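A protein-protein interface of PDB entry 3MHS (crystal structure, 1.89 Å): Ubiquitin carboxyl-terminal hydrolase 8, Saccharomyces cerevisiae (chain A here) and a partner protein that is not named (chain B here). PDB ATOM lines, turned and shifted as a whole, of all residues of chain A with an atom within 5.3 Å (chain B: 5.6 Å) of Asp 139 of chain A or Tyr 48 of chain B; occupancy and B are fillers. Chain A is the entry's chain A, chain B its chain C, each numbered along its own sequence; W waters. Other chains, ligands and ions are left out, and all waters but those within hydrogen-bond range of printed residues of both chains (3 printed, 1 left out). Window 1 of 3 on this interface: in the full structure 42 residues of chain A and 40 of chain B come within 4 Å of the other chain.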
ATOM      1  N   MET A 135      10.633  14.178 -34.281  1.00  0.00           N
ATOM      2  CA  MET A 135       9.402  13.814 -33.616  1.00  0.00           C
ATOM      3  C   MET A 135       9.240  14.507 -32.257  1.00  0.00           C
ATOM      4  O   MET A 135       8.195  15.061 -31.947  1.00  0.00           O
ATOM      5  CB  MET A 135       9.381  12.302 -33.384  1.00  0.00           C
ATOM      6  CG  MET A 135       8.040  11.774 -32.970  1.00  0.00           C
ATOM      7  SD  MET A 135       8.039   9.969 -32.852  1.00  0.00           S
ATOM      8  CE  MET A 135       8.677   9.741 -31.199  1.00  0.00           C
ATOM      9  N   GLU A 136      10.336  14.505 -31.512  1.00  0.00           N
ATOM     10  CA  GLU A 136      10.305  14.980 -30.133  1.00  0.00           C
ATOM     11  C   GLU A 136      10.199  16.510 -30.032  1.00  0.00           C
ATOM     12  O   GLU A 136       9.695  17.016 -29.022  1.00  0.00           O
ATOM     13  CB  GLU A 136      11.534  14.455 -29.368  1.00  0.00           C
ATOM     14  CG  GLU A 136      11.703  12.909 -29.347  1.00  0.00           C
ATOM     15  CD  GLU A 136      12.400  12.308 -30.601  1.00  0.00           C
ATOM     16  OE1 GLU A 136      12.637  11.077 -30.605  1.00  0.00           O
ATOM     17  OE2 GLU A 136      12.705  13.026 -31.581  1.00  0.00           O
ATOM     18  N   ARG A 137      10.621  17.228 -31.068  1.00  0.00           N
ATOM     19  CA  ARG A 137      10.631  18.690 -31.075  1.00  0.00           C
ATOM     20  C   ARG A 137       9.454  19.332 -31.834  1.00  0.00           C
ATOM     21  O   ARG A 137       9.286  20.567 -31.767  1.00  0.00           O
ATOM     22  CB  ARG A 137      11.941  19.175 -31.707  1.00  0.00           C
ATOM     23  CG  ARG A 137      13.219  18.706 -30.995  1.00  0.00           C
ATOM     24  CD  ARG A 137      13.409  19.449 -29.612  1.00  0.00           C
ATOM     25  NE  ARG A 137      12.872  18.703 -28.469  1.00  0.00           N
ATOM     26  CZ  ARG A 137      11.852  19.077 -27.670  1.00  0.00           C
ATOM     27  NH1 ARG A 137      11.145  20.218 -27.827  1.00  0.00           N
ATOM     28  NH2 ARG A 137      11.515  18.265 -26.673  1.00  0.00           N
ATOM     29  N   ARG A 138       8.633  18.520 -32.506  1.00  0.00           N
ATOM     30  CA  ARG A 138       7.705  19.039 -33.526  1.00  0.00           C
ATOM     31  C   ARG A 138       6.697  20.027 -32.991  1.00  0.00           C
ATOM     32  O   ARG A 138       6.229  20.881 -33.717  1.00  0.00           O
ATOM     33  CB  ARG A 138       6.966  17.903 -34.267  1.00  0.00           C
ATOM     34  CG  ARG A 138       5.890  17.216 -33.435  1.00  0.00           C
ATOM     35  CD  ARG A 138       5.411  15.900 -34.072  1.00  0.00           C
ATOM     36  NE  ARG A 138       4.229  15.392 -33.362  1.00  0.00           N
ATOM     37  CZ  ARG A 138       4.265  14.601 -32.295  1.00  0.00           C
ATOM     38  NH1 ARG A 138       5.412  14.205 -31.796  1.00  0.00           N
ATOM     39  NH2 ARG A 138       3.148  14.241 -31.693  1.00  0.00           N
ATOM     40  N   ASP A 139       6.325  19.873 -31.724  1.00  0.00           N
ATOM     41  CA  ASP A 139       5.370  20.736 -31.087  1.00  0.00           C
ATOM     42  C   ASP A 139       6.017  21.745 -30.138  1.00  0.00           C
ATOM     43  O   ASP A 139       5.318  22.530 -29.505  1.00  0.00           O
ATOM     44  CB  ASP A 139       4.340  19.914 -30.337  1.00  0.00           C
ATOM     45  CG  ASP A 139       3.502  19.052 -31.273  1.00  0.00           C
ATOM     46  OD1 ASP A 139       3.152  19.529 -32.376  1.00  0.00           O
ATOM     47  OD2 ASP A 139       3.238  17.915 -30.898  1.00  0.00           O
ATOM     48  N   GLY A 140       7.339  21.729 -30.066  1.00  0.00           N
ATOM     49  CA  GLY A 140       8.082  22.698 -29.270  1.00  0.00           C
ATOM     50  C   GLY A 140       7.859  22.583 -27.765  1.00  0.00           C
ATOM     51  O   GLY A 140       7.992  23.552 -27.027  1.00  0.00           O
ATOM     52  N   LEU A 141       7.523  21.393 -27.303  1.00  0.00           N
ATOM     53  CA  LEU A 141       7.201  21.201 -25.896  1.00  0.00           C
ATOM     54  C   LEU A 141       8.461  20.922 -25.119  1.00  0.00           C
ATOM     55  O   LEU A 141       9.181  19.987 -25.423  1.00  0.00           O
ATOM     56  CB  LEU A 141       6.215  20.038 -25.730  1.00  0.00           C
ATOM     57  CG  LEU A 141       4.882  20.299 -26.437  1.00  0.00           C
ATOM     58  CD1 LEU A 141       4.048  19.014 -26.434  1.00  0.00           C
ATOM     59  CD2 LEU A 141       4.120  21.451 -25.745  1.00  0.00           C
ATOM     60  N   HIS A 162       4.128  29.370 -27.601  1.00  0.00           N
ATOM     61  CA  HIS A 162       2.977  28.694 -28.170  1.00  0.00           C
ATOM     62  C   HIS A 162       1.938  29.663 -28.725  1.00  0.00           C
ATOM     63  O   HIS A 162       0.739  29.384 -28.741  1.00  0.00           O
ATOM     64  CB  HIS A 162       2.406  27.741 -27.138  1.00  0.00           C
ATOM     65  CG  HIS A 162       3.348  26.608 -26.877  1.00  0.00           C
ATOM     66  ND1 HIS A 162       4.107  26.511 -25.730  1.00  0.00           N
ATOM     67  CD2 HIS A 162       3.833  25.676 -27.726  1.00  0.00           C
ATOM     68  CE1 HIS A 162       4.908  25.454 -25.831  1.00  0.00           C
ATOM     69  NE2 HIS A 162       4.777  24.947 -27.041  1.00  0.00           N
ATOM     70  N   TYR A 200      12.081  23.854 -30.990  1.00  0.00           N
ATOM     71  CA  TYR A 200      11.552  23.297 -32.218  1.00  0.00           C
ATOM     72  C   TYR A 200      12.614  22.682 -33.144  1.00  0.00           C
ATOM     73  O   TYR A 200      12.295  21.878 -34.014  1.00  0.00           O
ATOM     74  CB  TYR A 200      10.808  24.380 -32.987  1.00  0.00           C
ATOM     75  CG  TYR A 200       9.485  24.770 -32.377  1.00  0.00           C
ATOM     76  CD1 TYR A 200       8.328  24.063 -32.658  1.00  0.00           C
ATOM     77  CD2 TYR A 200       9.379  25.899 -31.576  1.00  0.00           C
ATOM     78  CE1 TYR A 200       7.095  24.459 -32.127  1.00  0.00           C
ATOM     79  CE2 TYR A 200       8.147  26.302 -31.044  1.00  0.00           C
ATOM     80  CZ  TYR A 200       7.018  25.585 -31.343  1.00  0.00           C
ATOM     81  OH  TYR A 200       5.824  25.969 -30.813  1.00  0.00           O
ATOM     82  N   ILE A 439      -2.500  23.448 -28.159  1.00  0.00           N
ATOM     83  CA  ILE A 439      -1.907  23.349 -29.466  1.00  0.00           C
ATOM     84  C   ILE A 439      -2.857  22.632 -30.430  1.00  0.00           C
ATOM     85  O   ILE A 439      -3.942  22.097 -30.062  1.00  0.00           O
ATOM     86  CB  ILE A 439      -0.519  22.691 -29.394  1.00  0.00           C
ATOM     87  CG1 ILE A 439      -0.637  21.219 -29.018  1.00  0.00           C
ATOM     88  CG2 ILE A 439       0.383  23.424 -28.368  1.00  0.00           C
ATOM     89  CD1 ILE A 439       0.624  20.421 -29.321  1.00  0.00           C
ATOM     90  N   GLN A 443      -5.264  19.481 -27.699  1.00  0.00           N
ATOM     91  CA  GLN A 443      -4.609  19.025 -26.487  1.00  0.00           C
ATOM     92  C   GLN A 443      -4.008  20.215 -25.749  1.00  0.00           C
ATOM     93  O   GLN A 443      -3.403  21.085 -26.363  1.00  0.00           O
ATOM     94  CB  GLN A 443      -3.497  18.015 -26.812  1.00  0.00           C
ATOM     95  CG  GLN A 443      -2.486  17.767 -25.674  1.00  0.00           C
ATOM     96  CD  GLN A 443      -2.885  16.676 -24.704  1.00  0.00           C
ATOM     97  OE1 GLN A 443      -3.301  16.952 -23.576  1.00  0.00           O
ATOM     98  NE2 GLN A 443      -2.722  15.407 -25.128  1.00  0.00           N
ATOM     99  N   PHE A 445      -1.490  21.413 -22.559  1.00  0.00           N
ATOM    100  CA  PHE A 445      -0.347  21.054 -21.771  1.00  0.00           C
ATOM    101  C   PHE A 445      -0.193  22.080 -20.638  1.00  0.00           C
ATOM    102  O   PHE A 445      -0.460  23.264 -20.813  1.00  0.00           O
ATOM    103  CB  PHE A 445       0.896  20.983 -22.667  1.00  0.00           C
ATOM    104  CG  PHE A 445       0.782  19.933 -23.747  1.00  0.00           C
ATOM    105  CD1 PHE A 445       1.193  18.633 -23.509  1.00  0.00           C
ATOM    106  CD2 PHE A 445       0.265  20.247 -24.976  1.00  0.00           C
ATOM    107  CE1 PHE A 445       1.020  17.659 -24.469  1.00  0.00           C
ATOM    108  CE2 PHE A 445       0.075  19.282 -25.944  1.00  0.00           C
ATOM    109  CZ  PHE A 445       0.459  17.966 -25.673  1.00  0.00           C
ATOM    110  N   SER A 454       0.468  16.572 -19.895  1.00  0.00           N
ATOM    111  CA  SER A 454      -0.834  16.546 -20.562  1.00  0.00           C
ATOM    112  C   SER A 454      -1.909  16.828 -19.542  1.00  0.00           C
ATOM    113  O   SER A 454      -1.880  16.300 -18.427  1.00  0.00           O
ATOM    114  CB  SER A 454      -1.088  15.153 -21.181  1.00  0.00           C
ATOM    115  OG  SER A 454      -0.159  14.933 -22.212  1.00  0.00           O
ATOM    116  N   ARG B  46       4.723   8.070 -30.919  1.00  0.00           N
ATOM    117  CA  ARG B  46       4.037   7.746 -29.677  1.00  0.00           C
ATOM    118  C   ARG B  46       3.286   8.960 -29.147  1.00  0.00           C
ATOM    119  O   ARG B  46       3.664  10.106 -29.414  1.00  0.00           O
ATOM    120  CB  ARG B  46       5.019   7.238 -28.610  1.00  0.00           C
ATOM    121  CG  ARG B  46       6.306   8.043 -28.473  1.00  0.00           C
ATOM    122  CD  ARG B  46       6.851   7.948 -27.053  1.00  0.00           C
ATOM    123  NE  ARG B  46       6.347   9.035 -26.221  1.00  0.00           N
ATOM    124  CZ  ARG B  46       7.042  10.122 -25.903  1.00  0.00           C
ATOM    125  NH1 ARG B  46       8.290  10.273 -26.341  1.00  0.00           N
ATOM    126  NH2 ARG B  46       6.486  11.065 -25.151  1.00  0.00           N
ATOM    127  N   SER B  47       2.210   8.693 -28.422  1.00  0.00           N
ATOM    128  CA  SER B  47       1.412   9.720 -27.786  1.00  0.00           C
ATOM    129  C   SER B  47       2.183  10.328 -26.629  1.00  0.00           C
ATOM    130  O   SER B  47       3.064   9.708 -26.028  1.00  0.00           O
ATOM    131  CB  SER B  47       0.110   9.103 -27.264  1.00  0.00           C
ATOM    132  OG  SER B  47      -0.765   8.786 -28.334  1.00  0.00           O
ATOM    133  N   TYR B  48       1.900  11.588 -26.359  1.00  0.00           N
ATOM    134  CA  TYR B  48       2.401  12.196 -25.155  1.00  0.00           C
ATOM    135  C   TYR B  48       1.753  11.475 -23.973  1.00  0.00           C
ATOM    136  O   TYR B  48       0.560  11.171 -23.984  1.00  0.00           O
ATOM    137  CB  TYR B  48       2.088  13.688 -25.153  1.00  0.00           C
ATOM    138  CG  TYR B  48       2.767  14.454 -26.275  1.00  0.00           C
ATOM    139  CD1 TYR B  48       4.153  14.501 -26.376  1.00  0.00           C
ATOM    140  CD2 TYR B  48       2.022  15.126 -27.227  1.00  0.00           C
ATOM    141  CE1 TYR B  48       4.777  15.213 -27.390  1.00  0.00           C
ATOM    142  CE2 TYR B  48       2.631  15.831 -28.237  1.00  0.00           C
ATOM    143  CZ  TYR B  48       4.010  15.871 -28.318  1.00  0.00           C
ATOM    144  OH  TYR B  48       4.628  16.630 -29.305  1.00  0.00           O
ATOM    145  N   TYR B  49       2.555  11.177 -22.964  1.00  0.00           N
ATOM    146  CA  TYR B  49       2.074  10.503 -21.792  1.00  0.00           C
ATOM    147  C   TYR B  49       1.033  11.319 -21.032  1.00  0.00           C
ATOM    148  O   TYR B  49       1.243  12.514 -20.735  1.00  0.00           O
ATOM    149  CB  TYR B  49       3.224  10.194 -20.841  1.00  0.00           C
ATOM    150  CG  TYR B  49       2.851   9.162 -19.820  1.00  0.00           C
ATOM    151  CD1 TYR B  49       2.936   7.798 -20.118  1.00  0.00           C
ATOM    152  CD2 TYR B  49       2.364   9.531 -18.571  1.00  0.00           C
ATOM    153  CE1 TYR B  49       2.580   6.854 -19.183  1.00  0.00           C
ATOM    154  CE2 TYR B  49       2.002   8.587 -17.639  1.00  0.00           C
ATOM    155  CZ  TYR B  49       2.102   7.269 -17.947  1.00  0.00           C
ATOM    156  OH  TYR B  49       1.752   6.362 -16.994  1.00  0.00           O
ATOM    157  N   PHE B  50      -0.056  10.649 -20.683  1.00  0.00           N
ATOM    158  CA  PHE B  50      -1.073  11.220 -19.798  1.00  0.00           C
ATOM    159  C   PHE B  50      -1.145  10.457 -18.486  1.00  0.00           C
ATOM    160  O   PHE B  50      -1.360   9.241 -18.473  1.00  0.00           O
ATOM    161  CB  PHE B  50      -2.455  11.218 -20.451  1.00  0.00           C
ATOM    162  CG  PHE B  50      -3.545  11.744 -19.532  1.00  0.00           C
ATOM    163  CD1 PHE B  50      -3.609  13.100 -19.230  1.00  0.00           C
ATOM    164  CD2 PHE B  50      -4.467  10.880 -18.939  1.00  0.00           C
ATOM    165  CE1 PHE B  50      -4.583  13.593 -18.356  1.00  0.00           C
ATOM    166  CE2 PHE B  50      -5.460  11.362 -18.080  1.00  0.00           C
ATOM    167  CZ  PHE B  50      -5.523  12.736 -17.801  1.00  0.00           C
ATOM    168  N   ILE B  58       5.140  14.509 -20.025  1.00  0.00           N
ATOM    169  CA  ILE B  58       4.711  14.000 -21.335  1.00  0.00           C
ATOM    170  C   ILE B  58       5.581  12.843 -21.857  1.00  0.00           C
ATOM    171  O   ILE B  58       5.237  12.218 -22.844  1.00  0.00           O
ATOM    172  CB  ILE B  58       4.668  15.138 -22.372  1.00  0.00           C
ATOM    173  CG1 ILE B  58       6.046  15.801 -22.497  1.00  0.00           C
ATOM    174  CG2 ILE B  58       3.567  16.117 -21.991  1.00  0.00           C
ATOM    175  CD1 ILE B  58       6.261  16.746 -23.705  1.00  0.00           C
HETATM  176  O   HOH W   1       3.322  12.705 -29.359  1.00  0.00           O
HETATM  177  O   HOH W   2       1.922  14.126 -18.759  1.00  0.00           O
HETATM  178  O   HOH W   3       6.006  12.376 -29.646  1.00  0.00           O
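The backbone carbonyl oxygen (O) of Tyr 49 of chain B is in hydrogen-bond range of the side-chain hydroxyl (OG) of Ser 454 of chain A, 3.2 Å away.
OD2 of Asp 139 of chain A is in hydrogen-bond range of OH of Tyr 48 of chain B (2.5 Å).
The guanidinium group (NH2) of Arg 46 of chain B sits at hydrogen-bond distance from the backbone carbonyl oxygen (O) of Ile 58 of chain B (2.9 Å).
The guanidinium group (NH1) of Arg 137 of chain A lies within hydrogen-bond range of the backbone carbonyl oxygen (O) of Leu 141 of chain A, at 3.1 Å.
N of Tyr 49 of chain B is in hydrogen-bond range of O of Ile 58 of chain B (2.9 Å).
The guanidinium group of Arg 138 of chain A is in salt-bridge range of the side-chain carboxylate of Asp 139 of chain A (3.7 Å).
O of Met 135 of chain A is in hydrogen-bond range of NH1 of Arg 138 of chain A, at 2.9 Å.
The backbone carbonyl oxygen (O) of Asp 139 of chain A lies within hydrogen-bond range of a ring nitrogen (NE2) of His 162 of chain A, at 3.5 Å.
Among the printed residues, merely in contact across the chains: Met 135 of chain A with Arg 46 of chain B (3.99 Å), Arg 138 of chain A with Tyr 48 of chain B (3.6 Å), Leu 141 of chain A with Tyr 48 of chain B (3.7 Å), Leu 141 of chain A with Ile 58 of chain B (3.9 Å), Phe 445 of chain A with Tyr 48 of chain B (3.6 Å), Phe 445 of chain A with Ile 58 of chain B (3.8 Å), Ser 454 of chain A with Tyr 48 of chain B (3.9 Å), Ser 454 of chain A with Phe 50 of chain B (3.7 Å) and Ser 454 of chain A with Ile 58 of chain B (3.8 Å).
Of chain B, only Tyr 48 comes within 4 Å of Asp 139 of chain A.
Tyr 48 of chain B touches five residues of chain A.
Of the printed residues of chain A, Tyr 49 of chain B touches Ser 454 (3.2 Å).
Of the printed residues of chain A, Arg 46 of chain B touches Met 135.
The nearest residue of chain A that does not touch Tyr 48 of chain B is Met 135 of chain A (4.7 Å).
Of the 13 printed residues of chain A, 6 touch a printed residue of chain B.
Of the 6 printed residues of chain B, 5 touch a printed residue of chain A.
Hydrophobic or aromatic side chains of chain B that line the printed part of chain A: Tyr 48, Phe 50 and Ile 58.
Among the printed residues, no Asp or Glu carboxylate lies within 4 Å of a Lys or Arg side-chain nitrogen of the other chain.
Water W1 bridges O of Arg 46 of chain B (2.6 Å) and NH2 of Arg 138 of chain A (2.8 Å).
Water W2 lies within hydrogen-bond range of O of Tyr 49 of chain B, N of Ser 454 of chain A and N of Ile 58 of chain B.
Water W3 lies within hydrogen-bond range of the guanidinium group of Arg 138 of chain A (2.9 Å) and the backbone carbonyl oxygen of Arg 46 of chain B (3.3 Å).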
